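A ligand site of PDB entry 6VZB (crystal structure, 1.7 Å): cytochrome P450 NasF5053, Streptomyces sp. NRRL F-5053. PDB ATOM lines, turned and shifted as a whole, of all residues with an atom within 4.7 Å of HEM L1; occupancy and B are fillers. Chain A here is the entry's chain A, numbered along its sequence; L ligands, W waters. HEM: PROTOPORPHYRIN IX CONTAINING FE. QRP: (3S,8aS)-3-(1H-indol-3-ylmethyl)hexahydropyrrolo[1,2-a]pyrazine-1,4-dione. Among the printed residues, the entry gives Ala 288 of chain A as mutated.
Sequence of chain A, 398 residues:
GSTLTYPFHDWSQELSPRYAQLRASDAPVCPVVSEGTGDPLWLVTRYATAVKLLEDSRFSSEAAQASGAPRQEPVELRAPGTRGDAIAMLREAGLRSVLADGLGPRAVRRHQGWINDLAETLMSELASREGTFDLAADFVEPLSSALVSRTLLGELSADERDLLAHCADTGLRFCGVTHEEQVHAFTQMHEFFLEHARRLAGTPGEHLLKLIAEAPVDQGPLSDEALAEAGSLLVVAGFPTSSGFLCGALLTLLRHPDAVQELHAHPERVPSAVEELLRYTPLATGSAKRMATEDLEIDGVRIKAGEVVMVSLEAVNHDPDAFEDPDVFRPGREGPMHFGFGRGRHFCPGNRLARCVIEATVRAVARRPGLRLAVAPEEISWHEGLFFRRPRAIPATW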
ATOM      1  N   SER A  61      14.961  18.868  34.015  1.00  0.00           N
ATOM      2  CA  SER A  61      14.062  19.424  33.024  1.00  0.00           C
ATOM      3  C   SER A  61      13.305  18.330  32.282  1.00  0.00           C
ATOM      4  O   SER A  61      12.092  18.428  32.059  1.00  0.00           O
ATOM      5  CB  SER A  61      14.867  20.278  32.041  1.00  0.00           C
ATOM      6  OG  SER A  61      13.983  20.965  31.176  1.00  0.00           O
ATOM      7  N   GLN A  65       9.226  17.674  31.720  1.00  0.00           N
ATOM      8  CA  GLN A  65       8.617  17.678  30.401  1.00  0.00           C
ATOM      9  C   GLN A  65       7.860  16.397  30.105  1.00  0.00           C
ATOM     10  O   GLN A  65       7.013  16.366  29.209  1.00  0.00           O
ATOM     11  CB  GLN A  65       9.674  17.841  29.316  1.00  0.00           C
ATOM     12  CG  GLN A  65      10.465  19.181  29.342  1.00  0.00           C
ATOM     13  CD  GLN A  65      11.690  19.129  28.435  1.00  0.00           C
ATOM     14  OE1 GLN A  65      12.816  19.532  28.814  1.00  0.00           O
ATOM     15  NE2 GLN A  65      11.498  18.586  27.254  1.00  0.00           N
ATOM     16  N   ILE A  87      15.296  17.563  21.931  1.00  0.00           N
ATOM     17  CA  ILE A  87      16.669  18.039  22.131  1.00  0.00           C
ATOM     18  C   ILE A  87      17.452  17.024  22.950  1.00  0.00           C
ATOM     19  O   ILE A  87      18.620  16.744  22.671  1.00  0.00           O
ATOM     20  CB  ILE A  87      16.716  19.451  22.748  1.00  0.00           C
ATOM     21  CG1 ILE A  87      18.151  19.994  22.715  1.00  0.00           C
ATOM     22  CG2 ILE A  87      16.281  19.462  24.207  1.00  0.00           C
ATOM     23  CD1 ILE A  87      18.690  20.234  21.317  1.00  0.00           C
ATOM     24  N   ARG A  91      20.806  15.054  21.472  1.00  0.00           N
ATOM     25  CA  ARG A  91      22.025  14.899  22.253  1.00  0.00           C
ATOM     26  C   ARG A  91      22.206  13.433  22.637  1.00  0.00           C
ATOM     27  O   ARG A  91      23.321  12.897  22.605  1.00  0.00           O
ATOM     28  CB  ARG A  91      21.970  15.803  23.494  1.00  0.00           C
ATOM     29  CG  ARG A  91      21.905  17.320  23.204  1.00  0.00           C
ATOM     30  CD  ARG A  91      21.369  18.155  24.391  1.00  0.00           C
ATOM     31  NE  ARG A  91      21.449  19.612  24.151  1.00  0.00           N
ATOM     32  CZ  ARG A  91      20.826  20.543  24.905  1.00  0.00           C
ATOM     33  NH1 ARG A  91      20.088  20.189  25.925  1.00  0.00           N
ATOM     34  NH2 ARG A  91      20.959  21.844  24.620  1.00  0.00           N
ATOM     35  N   LEU A 103      24.091  25.746  15.259  1.00  0.00           N
ATOM     36  CA  LEU A 103      23.586  26.821  16.096  1.00  0.00           C
ATOM     37  C   LEU A 103      24.647  27.751  16.657  1.00  0.00           C
ATOM     38  O   LEU A 103      24.317  28.861  17.079  1.00  0.00           O
ATOM     39  CB  LEU A 103      22.763  26.257  17.265  1.00  0.00           C
ATOM     40  CG  LEU A 103      21.560  25.420  16.840  1.00  0.00           C
ATOM     41  CD1 LEU A 103      21.016  24.706  18.054  1.00  0.00           C
ATOM     42  CD2 LEU A 103      20.474  26.277  16.192  1.00  0.00           C
ATOM     43  N   LEU A 147      14.718  33.510   9.261  1.00  0.00           N
ATOM     44  CA  LEU A 147      15.624  32.811  10.188  1.00  0.00           C
ATOM     45  C   LEU A 147      15.251  31.335  10.293  1.00  0.00           C
ATOM     46  O   LEU A 147      16.113  30.460  10.158  1.00  0.00           O
ATOM     47  CB  LEU A 147      15.599  33.477  11.563  1.00  0.00           C
ATOM     48  CG  LEU A 147      16.365  32.795  12.698  1.00  0.00           C
ATOM     49  CD1 LEU A 147      17.845  32.972  12.449  1.00  0.00           C
ATOM     50  CD2 LEU A 147      15.936  33.344  14.058  1.00  0.00           C
ATOM     51  N   LEU A 152      17.169  26.943  10.273  1.00  0.00           N
ATOM     52  CA  LEU A 152      16.614  25.812  11.010  1.00  0.00           C
ATOM     53  C   LEU A 152      16.042  24.718  10.120  1.00  0.00           C
ATOM     54  O   LEU A 152      16.555  23.605  10.133  1.00  0.00           O
ATOM     55  CB  LEU A 152      15.558  26.265  12.019  1.00  0.00           C
ATOM     56  CG  LEU A 152      16.082  27.334  12.985  1.00  0.00           C
ATOM     57  CD1 LEU A 152      14.979  27.708  13.972  1.00  0.00           C
ATOM     58  CD2 LEU A 152      17.437  26.934  13.665  1.00  0.00           C
ATOM     59  N   LEU A 233      10.554  20.558  17.174  1.00  0.00           N
ATOM     60  CA  LEU A 233      11.314  21.251  18.221  1.00  0.00           C
ATOM     61  C   LEU A 233      11.821  22.597  17.699  1.00  0.00           C
ATOM     62  O   LEU A 233      11.772  23.619  18.394  1.00  0.00           O
ATOM     63  CB  LEU A 233      12.485  20.385  18.678  1.00  0.00           C
ATOM     64  CG  LEU A 233      13.584  21.142  19.443  1.00  0.00           C
ATOM     65  CD1 LEU A 233      13.035  21.581  20.770  1.00  0.00           C
ATOM     66  CD2 LEU A 233      14.873  20.338  19.600  1.00  0.00           C
ATOM     67  N   LEU A 234      12.333  22.611  16.474  1.00  0.00           N
ATOM     68  CA  LEU A 234      12.857  23.843  15.944  1.00  0.00           C
ATOM     69  C   LEU A 234      11.751  24.861  15.745  1.00  0.00           C
ATOM     70  O   LEU A 234      11.992  26.060  15.928  1.00  0.00           O
ATOM     71  CB  LEU A 234      13.619  23.550  14.662  1.00  0.00           C
ATOM     72  CG  LEU A 234      14.834  22.670  14.922  1.00  0.00           C
ATOM     73  CD1 LEU A 234      15.582  22.425  13.606  1.00  0.00           C
ATOM     74  CD2 LEU A 234      15.753  23.296  15.967  1.00  0.00           C
ATOM     75  N   ALA A 237      10.612  25.937  19.584  1.00  0.00           N
ATOM     76  CA  ALA A 237      11.677  26.607  20.310  1.00  0.00           C
ATOM     77  C   ALA A 237      12.211  27.834  19.592  1.00  0.00           C
ATOM     78  O   ALA A 237      12.795  28.698  20.243  1.00  0.00           O
ATOM     79  CB  ALA A 237      12.827  25.641  20.547  1.00  0.00           C
ATOM     80  N   GLY A 238      12.071  27.919  18.279  1.00  0.00           N
ATOM     81  CA  GLY A 238      12.732  28.957  17.507  1.00  0.00           C
ATOM     82  C   GLY A 238      11.827  29.998  16.883  1.00  0.00           C
ATOM     83  O   GLY A 238      12.270  31.122  16.608  1.00  0.00           O
ATOM     84  N   THR A 241       9.140  32.121  19.788  1.00  0.00           N
ATOM     85  CA  THR A 241      10.087  32.780  20.674  1.00  0.00           C
ATOM     86  C   THR A 241      10.748  33.970  19.974  1.00  0.00           C
ATOM     87  O   THR A 241      10.712  35.102  20.481  1.00  0.00           O
ATOM     88  CB  THR A 241      11.119  31.760  21.133  1.00  0.00           C
ATOM     89  OG1 THR A 241      11.670  31.131  19.964  1.00  0.00           O
ATOM     90  CG2 THR A 241      10.499  30.676  22.018  1.00  0.00           C
ATOM     91  N   SER A 242      11.353  33.721  18.819  1.00  0.00           N
ATOM     92  CA  SER A 242      12.005  34.814  18.095  1.00  0.00           C
ATOM     93  C   SER A 242      11.000  35.875  17.664  1.00  0.00           C
ATOM     94  O   SER A 242      11.275  37.078  17.767  1.00  0.00           O
ATOM     95  CB  SER A 242      12.767  34.288  16.876  1.00  0.00           C
ATOM     96  OG  SER A 242      13.727  33.338  17.250  1.00  0.00           O
ATOM     97  N   PHE A 245       9.793  37.793  20.816  1.00  0.00           N
ATOM     98  CA  PHE A 245      10.822  38.622  21.409  1.00  0.00           C
ATOM     99  C   PHE A 245      11.132  39.817  20.509  1.00  0.00           C
ATOM    100  O   PHE A 245      11.264  40.955  21.006  1.00  0.00           O
ATOM    101  CB  PHE A 245      12.099  37.844  21.679  1.00  0.00           C
ATOM    102  CG  PHE A 245      13.086  38.684  22.447  1.00  0.00           C
ATOM    103  CD1 PHE A 245      12.934  38.840  23.813  1.00  0.00           C
ATOM    104  CD2 PHE A 245      14.049  39.426  21.807  1.00  0.00           C
ATOM    105  CE1 PHE A 245      13.778  39.673  24.525  1.00  0.00           C
ATOM    106  CE2 PHE A 245      14.894  40.256  22.533  1.00  0.00           C
ATOM    107  CZ  PHE A 245      14.765  40.378  23.877  1.00  0.00           C
ATOM    108  N   LEU A 278      17.269  41.627  26.414  1.00  0.00           N
ATOM    109  CA  LEU A 278      17.018  40.251  26.839  1.00  0.00           C
ATOM    110  C   LEU A 278      16.637  40.192  28.319  1.00  0.00           C
ATOM    111  O   LEU A 278      15.894  39.290  28.729  1.00  0.00           O
ATOM    112  CB  LEU A 278      18.245  39.377  26.552  1.00  0.00           C
ATOM    113  CG  LEU A 278      18.338  38.997  25.072  1.00  0.00           C
ATOM    114  CD1 LEU A 278      19.789  38.736  24.683  1.00  0.00           C
ATOM    115  CD2 LEU A 278      17.465  37.828  24.663  1.00  0.00           C
ATOM    116  N   LEU A 283       9.098  37.807  27.841  1.00  0.00           N
ATOM    117  CA  LEU A 283       8.695  36.932  26.745  1.00  0.00           C
ATOM    118  C   LEU A 283       7.708  35.896  27.228  1.00  0.00           C
ATOM    119  O   LEU A 283       6.518  35.972  26.892  1.00  0.00           O
ATOM    120  CB  LEU A 283       9.894  36.250  26.099  1.00  0.00           C
ATOM    121  CG  LEU A 283       9.641  35.386  24.865  1.00  0.00           C
ATOM    122  CD1 LEU A 283       8.998  36.143  23.749  1.00  0.00           C
ATOM    123  CD2 LEU A 283      10.931  34.829  24.357  1.00  0.00           C
ATOM    124  N   ALA A 288      10.108  28.553  33.191  1.00  0.00           N
ATOM    125  CA  ALA A 288      10.952  27.375  33.098  1.00  0.00           C
ATOM    126  C   ALA A 288      10.695  26.492  34.309  1.00  0.00           C
ATOM    127  O   ALA A 288      10.327  26.991  35.378  1.00  0.00           O
ATOM    128  CB  ALA A 288      12.412  27.783  33.025  1.00  0.00           C
ATOM    129  N   ARG A 290      11.465  22.455  36.477  1.00  0.00           N
ATOM    130  CA  ARG A 290      12.301  21.289  36.725  1.00  0.00           C
ATOM    131  C   ARG A 290      11.624  20.393  37.755  1.00  0.00           C
ATOM    132  O   ARG A 290      10.963  20.875  38.675  1.00  0.00           O
ATOM    133  CB  ARG A 290      13.676  21.682  37.270  1.00  0.00           C
ATOM    134  CG  ARG A 290      14.423  22.724  36.432  1.00  0.00           C
ATOM    135  CD  ARG A 290      14.989  22.165  35.125  1.00  0.00           C
ATOM    136  NE  ARG A 290      15.865  23.116  34.425  1.00  0.00           N
ATOM    137  CZ  ARG A 290      15.490  23.937  33.446  1.00  0.00           C
ATOM    138  NH1 ARG A 290      14.221  23.977  33.004  1.00  0.00           N
ATOM    139  NH2 ARG A 290      16.379  24.733  32.897  1.00  0.00           N
ATOM    140  N   LEU A 313      11.449  33.468  34.535  1.00  0.00           N
ATOM    141  CA  LEU A 313      12.639  34.195  34.117  1.00  0.00           C
ATOM    142  C   LEU A 313      12.380  35.692  34.094  1.00  0.00           C
ATOM    143  O   LEU A 313      13.282  36.496  34.403  1.00  0.00           O
ATOM    144  CB  LEU A 313      13.089  33.677  32.755  1.00  0.00           C
ATOM    145  CG  LEU A 313      13.275  32.160  32.676  1.00  0.00           C
ATOM    146  CD1 LEU A 313      13.828  31.775  31.315  1.00  0.00           C
ATOM    147  CD2 LEU A 313      14.197  31.673  33.823  1.00  0.00           C
ATOM    148  N   PHE A 339      18.697  36.325  32.761  1.00  0.00           N
ATOM    149  CA  PHE A 339      18.119  34.998  32.575  1.00  0.00           C
ATOM    150  C   PHE A 339      17.268  34.900  31.321  1.00  0.00           C
ATOM    151  O   PHE A 339      16.421  33.997  31.222  1.00  0.00           O
ATOM    152  CB  PHE A 339      17.241  34.630  33.776  1.00  0.00           C
ATOM    153  CG  PHE A 339      17.958  33.999  34.914  1.00  0.00           C
ATOM    154  CD1 PHE A 339      19.018  34.631  35.554  1.00  0.00           C
ATOM    155  CD2 PHE A 339      17.558  32.781  35.394  1.00  0.00           C
ATOM    156  CE1 PHE A 339      19.640  34.041  36.631  1.00  0.00           C
ATOM    157  CE2 PHE A 339      18.182  32.186  36.462  1.00  0.00           C
ATOM    158  CZ  PHE A 339      19.209  32.825  37.090  1.00  0.00           C
ATOM    159  N   GLY A 340      17.430  35.815  30.356  1.00  0.00           N
ATOM    160  CA  GLY A 340      16.554  35.746  29.186  1.00  0.00           C
ATOM    161  C   GLY A 340      16.774  34.515  28.340  1.00  0.00           C
ATOM    162  O   GLY A 340      15.889  34.167  27.563  1.00  0.00           O
ATOM    163  N   PHE A 341      17.945  33.888  28.440  1.00  0.00           N
ATOM    164  CA  PHE A 341      18.234  32.607  27.813  1.00  0.00           C
ATOM    165  C   PHE A 341      18.311  31.473  28.832  1.00  0.00           C
ATOM    166  O   PHE A 341      18.744  30.356  28.500  1.00  0.00           O
ATOM    167  CB  PHE A 341      19.541  32.709  27.035  1.00  0.00           C
ATOM    168  CG  PHE A 341      19.469  33.570  25.791  1.00  0.00           C
ATOM    169  CD1 PHE A 341      18.474  33.356  24.841  1.00  0.00           C
ATOM    170  CD2 PHE A 341      20.402  34.577  25.555  1.00  0.00           C
ATOM    171  CE1 PHE A 341      18.424  34.106  23.697  1.00  0.00           C
ATOM    172  CE2 PHE A 341      20.353  35.325  24.389  1.00  0.00           C
ATOM    173  CZ  PHE A 341      19.354  35.089  23.464  1.00  0.00           C
ATOM    174  N   GLY A 342      17.872  31.719  30.055  1.00  0.00           N
ATOM    175  CA  GLY A 342      17.969  30.711  31.083  1.00  0.00           C
ATOM    176  C   GLY A 342      19.263  30.683  31.851  1.00  0.00           C
ATOM    177  O   GLY A 342      19.983  31.679  31.992  1.00  0.00           O
ATOM    178  N   HIS A 346      20.707  23.929  30.500  1.00  0.00           N
ATOM    179  CA  HIS A 346      19.670  24.106  29.496  1.00  0.00           C
ATOM    180  C   HIS A 346      19.640  25.517  28.955  1.00  0.00           C
ATOM    181  O   HIS A 346      18.622  25.933  28.386  1.00  0.00           O
ATOM    182  CB  HIS A 346      18.301  23.739  30.088  1.00  0.00           C
ATOM    183  CG  HIS A 346      18.226  22.309  30.505  1.00  0.00           C
ATOM    184  ND1 HIS A 346      18.181  21.283  29.596  1.00  0.00           N
ATOM    185  CD2 HIS A 346      18.255  21.740  31.735  1.00  0.00           C
ATOM    186  CE1 HIS A 346      18.144  20.122  30.252  1.00  0.00           C
ATOM    187  NE2 HIS A 346      18.195  20.375  31.546  1.00  0.00           N
ATOM    188  N   CYS A 348      19.732  28.437  26.540  1.00  0.00           N
ATOM    189  CA  CYS A 348      19.214  28.427  25.181  1.00  0.00           C
ATOM    190  C   CYS A 348      20.311  28.174  24.152  1.00  0.00           C
ATOM    191  O   CYS A 348      21.205  29.003  23.983  1.00  0.00           O
ATOM    192  CB  CYS A 348      18.526  29.762  24.861  1.00  0.00           C
ATOM    193  SG  CYS A 348      18.078  29.844  23.122  1.00  0.00           S
ATOM    194  N   PRO A 349      20.269  27.049  23.439  1.00  0.00           N
ATOM    195  CA  PRO A 349      21.268  26.807  22.378  1.00  0.00           C
ATOM    196  C   PRO A 349      21.069  27.666  21.165  1.00  0.00           C
ATOM    197  O   PRO A 349      22.002  27.785  20.355  1.00  0.00           O
ATOM    198  CB  PRO A 349      21.096  25.320  22.045  1.00  0.00           C
ATOM    199  CG  PRO A 349      19.727  24.972  22.503  1.00  0.00           C
ATOM    200  CD  PRO A 349      19.377  25.889  23.637  1.00  0.00           C
ATOM    201  N   GLY A 350      19.886  28.242  20.997  1.00  0.00           N
ATOM    202  CA  GLY A 350      19.602  29.209  19.972  1.00  0.00           C
ATOM    203  C   GLY A 350      20.090  30.601  20.288  1.00  0.00           C
ATOM    204  O   GLY A 350      19.793  31.538  19.545  1.00  0.00           O
ATOM    205  N   ALA A 354      19.700  33.878  18.009  1.00  0.00           N
ATOM    206  CA  ALA A 354      18.811  34.877  18.580  1.00  0.00           C
ATOM    207  C   ALA A 354      19.544  36.217  18.736  1.00  0.00           C
ATOM    208  O   ALA A 354      19.064  37.257  18.269  1.00  0.00           O
ATOM    209  CB  ALA A 354      18.259  34.393  19.924  1.00  0.00           C
HETATM  210  CHA HEM L   1      15.727  26.814  25.510  1.00  0.00           C
HETATM  211  CHB HEM L   1      14.980  31.595  25.214  1.00  0.00           C
HETATM  212  CHC HEM L   1      15.371  31.384  20.419  1.00  0.00           C
HETATM  213  CHD HEM L   1      16.354  26.686  20.698  1.00  0.00           C
HETATM  214  C1A HEM L   1      15.554  28.130  25.854  1.00  0.00           C
HETATM  215  C2A HEM L   1      15.410  28.649  27.195  1.00  0.00           C
HETATM  216  C3A HEM L   1      15.213  29.970  27.094  1.00  0.00           C
HETATM  217  C4A HEM L   1      15.195  30.334  25.695  1.00  0.00           C
HETATM  218  CMA HEM L   1      15.006  30.960  28.253  1.00  0.00           C
HETATM  219  CAA HEM L   1      15.553  27.852  28.501  1.00  0.00           C
HETATM  220  CBA HEM L   1      14.297  27.130  28.935  1.00  0.00           C
HETATM  221  CGA HEM L   1      14.547  26.330  30.209  1.00  0.00           C
HETATM  222  O1A HEM L   1      13.863  25.278  30.403  1.00  0.00           O
HETATM  223  O2A HEM L   1      15.399  26.704  31.071  1.00  0.00           O
HETATM  224  C1B HEM L   1      14.998  31.969  23.903  1.00  0.00           C
HETATM  225  C2B HEM L   1      14.746  33.284  23.391  1.00  0.00           C
HETATM  226  C3B HEM L   1      14.862  33.229  22.074  1.00  0.00           C
HETATM  227  C4B HEM L   1      15.130  31.854  21.696  1.00  0.00           C
HETATM  228  CMB HEM L   1      14.484  34.551  24.216  1.00  0.00           C
HETATM  229  CAB HEM L   1      14.665  34.462  21.156  1.00  0.00           C
HETATM  230  CBB HEM L   1      14.929  34.470  19.848  1.00  0.00           C
HETATM  231  C1C HEM L   1      15.729  30.114  20.081  1.00  0.00           C
HETATM  232  C2C HEM L   1      16.026  29.639  18.738  1.00  0.00           C
HETATM  233  C3C HEM L   1      16.319  28.347  18.858  1.00  0.00           C
HETATM  234  C4C HEM L   1      16.197  27.961  20.248  1.00  0.00           C
HETATM  235  CMC HEM L   1      16.058  30.509  17.478  1.00  0.00           C
HETATM  236  CAC HEM L   1      16.714  27.280  17.830  1.00  0.00           C
HETATM  237  CBC HEM L   1      16.583  27.492  16.549  1.00  0.00           C
HETATM  238  C1D HEM L   1      16.164  26.296  21.988  1.00  0.00           C
HETATM  239  C2D HEM L   1      16.177  24.943  22.476  1.00  0.00           C
HETATM  240  C3D HEM L   1      15.990  24.987  23.807  1.00  0.00           C
HETATM  241  C4D HEM L   1      15.889  26.362  24.203  1.00  0.00           C
HETATM  242  CMD HEM L   1      16.310  23.692  21.585  1.00  0.00           C
HETATM  243  CAD HEM L   1      15.889  23.785  24.787  1.00  0.00           C
HETATM  244  CBD HEM L   1      17.139  23.594  25.611  1.00  0.00           C
HETATM  245  CGD HEM L   1      16.983  22.492  26.648  1.00  0.00           C
HETATM  246  O1D HEM L   1      17.988  21.795  26.969  1.00  0.00           O
HETATM  247  O2D HEM L   1      15.845  22.299  27.138  1.00  0.00           O
HETATM  248  NA  HEM L   1      15.407  29.175  24.970  1.00  0.00           N
HETATM  249  NB  HEM L   1      15.213  31.097  22.852  1.00  0.00           N
HETATM  250  NC  HEM L   1      15.865  29.068  20.986  1.00  0.00           N
HETATM  251  ND  HEM L   1      15.984  27.154  23.057  1.00  0.00           N
HETATM  252 FE   HEM L   1      15.815  29.185  22.983  1.00  0.00          FE
HETATM  253  C   QRP L   2      10.508  22.229  27.342  1.00  0.00           C
HETATM  254  N   QRP L   2      12.938  22.279  26.553  1.00  0.00           N
HETATM  255  O   QRP L   2       9.649  22.461  28.153  1.00  0.00           O
HETATM  256  CA  QRP L   2      11.945  22.609  27.523  1.00  0.00           C
HETATM  257  CB  QRP L   2      11.938  24.222  27.610  1.00  0.00           C
HETATM  258  CG  QRP L   2      11.447  24.928  26.287  1.00  0.00           C
HETATM  259  OAA QRP L   2      13.452  21.397  24.493  1.00  0.00           O
HETATM  260  CAH QRP L   2       8.936  21.727  24.116  1.00  0.00           C
HETATM  261  CAI QRP L   2      10.493  21.963  23.812  1.00  0.00           C
HETATM  262  CAJ QRP L   2       8.834  21.165  25.392  1.00  0.00           C
HETATM  263  CAN QRP L   2      12.620  21.676  25.305  1.00  0.00           C
HETATM  264  CAT QRP L   2      11.107  21.304  25.113  1.00  0.00           C
HETATM  265  NAU QRP L   2      10.194  21.621  26.050  1.00  0.00           N
HETATM  266  CD1 QRP L   2      12.396  25.425  25.398  1.00  0.00           C
HETATM  267  CD2 QRP L   2      10.217  25.213  25.747  1.00  0.00           C
HETATM  268  NE1 QRP L   2      11.731  25.983  24.330  1.00  0.00           N
HETATM  269  CE2 QRP L   2      10.374  25.856  24.542  1.00  0.00           C
HETATM  270  CE3 QRP L   2       8.917  24.941  26.211  1.00  0.00           C
HETATM  271  CH2 QRP L   2       7.952  25.983  24.264  1.00  0.00           C
HETATM  272  CZ2 QRP L   2       9.241  26.258  23.808  1.00  0.00           C
HETATM  273  CZ3 QRP L   2       7.792  25.352  25.485  1.00  0.00           C
HETATM  274  C   QRP L   3       8.402  26.343  29.466  1.00  0.00           C
HETATM  275  N   QRP L   3       8.125  28.810  29.306  1.00  0.00           N
HETATM  276  O   QRP L   3       9.057  25.448  29.885  1.00  0.00           O
HETATM  277  CA  QRP L   3       8.928  27.655  28.995  1.00  0.00           C
HETATM  278  CB  QRP L   3      10.354  27.884  29.608  1.00  0.00           C
HETATM  279  CG  QRP L   3      10.830  29.269  29.029  1.00  0.00           C
HETATM  280  OAA QRP L   3       6.003  29.674  29.422  1.00  0.00           O
HETATM  281  CAH QRP L   3       4.725  25.513  29.432  1.00  0.00           C
HETATM  282  CAI QRP L   3       4.789  27.079  29.458  1.00  0.00           C
HETATM  283  CAJ QRP L   3       6.012  25.054  29.721  1.00  0.00           C
HETATM  284  CAN QRP L   3       6.716  28.750  29.208  1.00  0.00           C
HETATM  285  CAT QRP L   3       6.233  27.318  28.834  1.00  0.00           C
HETATM  286  NAU QRP L   3       6.971  26.258  29.342  1.00  0.00           N
HETATM  287  CD1 QRP L   3      10.856  30.364  29.866  1.00  0.00           C
HETATM  288  CD2 QRP L   3      11.149  29.681  27.769  1.00  0.00           C
HETATM  289  NE1 QRP L   3      11.222  31.462  29.126  1.00  0.00           N
HETATM  290  CE2 QRP L   3      11.399  31.030  27.822  1.00  0.00           C
HETATM  291  CE3 QRP L   3      11.255  28.969  26.564  1.00  0.00           C
HETATM  292  CH2 QRP L   3      11.868  31.000  25.452  1.00  0.00           C
HETATM  293  CZ2 QRP L   3      11.747  31.695  26.639  1.00  0.00           C
HETATM  294  CZ3 QRP L   3      11.616  29.627  25.401  1.00  0.00           C
HETATM  295  O   HOH W   1      15.476  19.550  27.582  1.00  0.00           O
HETATM  296  O   HOH W   2      14.864  22.747  29.636  1.00  0.00           O
HETATM  297  O   HOH W   3      11.424  24.771  31.226  1.00  0.00           O
HETATM  298  O   HOH W   4      13.223  28.176  22.864  1.00  0.00           O
HETATM  299  O   HOH W   5      18.005  27.390  31.120  1.00  0.00           O
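An iron atom (FE) of HEM L1 is bound by the side-chain sulfur of Cys 348, 2.4 Å away.
NH1 of Arg 91 lies within salt-bridge range of O1D of HEM L1 (2.8 Å).
The guanidinium group (NH2) of Arg 290 is in salt-bridge range of an oxygen (O2A) of HEM L1 (2.9 Å).
An oxygen (O1D) of HEM L1 sits at hydrogen-bond distance from a ring nitrogen (ND1) of His 346 (2.7 Å).
A nitrogen (N) of QRP L2 is in hydrogen-bond range of an oxygen (O2D) of HEM L1, 3.0 Å away.
The backbone carbonyl oxygen (O) of Ala 237 sits at hydrogen-bond distance from the side-chain hydroxyl (OG1) of Thr 241 (2.7 Å).
N of Cys 348 lies within hydrogen-bond range of O of Phe 341, 2.9 Å away.
The side-chain hydroxyl (OG) of Ser 242 lies within hydrogen-bond range of the backbone carbonyl oxygen (O) of Gly 238 (2.7 Å).
OG1 of Thr 241 lies close to O of Gly 238 (3.4 Å).
The side-chain sulfur (SG) of Cys 348 sits close to the backbone NH (N) of Gly 350 (3.2 Å).
O of Ala 237 lies close to NC of HEM L1 (3.2 Å).
Ile 87 touches HEM L1.
Leu 152 touches HEM L1.
Leu 233 touches HEM L1 (CD1 to CMD, 3.98 Å).
Gly 238 touches HEM L1 (CA to C2C, 3.6 Å).
OG1 of Thr 241 touches CHC of HEM L1 (3.7 Å).
Ser 242 touches HEM L1 (OG to CBB, 3.1 Å).
Leu 283 touches HEM L1 (CD2 to CMB, 3.6 Å).
Ala 288 touches HEM L1 (CB to O2A, 3.7 Å).
Leu 313 touches HEM L1.
Gly 340 touches HEM L1.
C of Phe 341 touches CMA of HEM L1, 3.4 Å away.
N of Gly 342 touches CMA of HEM L1 (3.5 Å).
CD of Pro 349 touches C3D of HEM L1, 3.5 Å away.
CA of Gly 350 touches C3C of HEM L1, 3.6 Å away.
CB of Ala 354 touches CBB of HEM L1 (3.3 Å).
Hydrophobic or aromatic side chains that line HEM L1: Ile 87, Leu 152, Leu 233, Ala 237, Leu 283, Ala 288, Leu 313, Phe 341, His 346, Pro 349 and Ala 354.
Of the 28 residues printed, 20 come within 4 Å of HEM L1.
The nearest printed residue that does not touch HEM L1 is Leu 103 (4.1 Å).
Water W3 lies within hydrogen-bond range of O1A of HEM L1 (2.6 Å), O of QRP L3 (2.8 Å) and NH1 of Arg 290 (3.4 Å).
Water W5 lies within hydrogen-bond range of O2A of HEM L1 (2.7 Å) and O of His 346 (3.2 Å).
Water W2 lies within hydrogen-bond range of the side-chain hydroxyl of Ser 61 (2.5 Å) and an oxygen (O2D) of HEM L1 (2.7 Å).
Water W4 lies within hydrogen-bond range of O of Ala 237 (2.7 Å) and NE1 of QRP L2 (3.0 Å).
Water W1 bridges an oxygen (O2D) of HEM L1 (2.8 Å) and the side-chain amide oxygen (OE1) of Gln 65 (2.9 Å).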
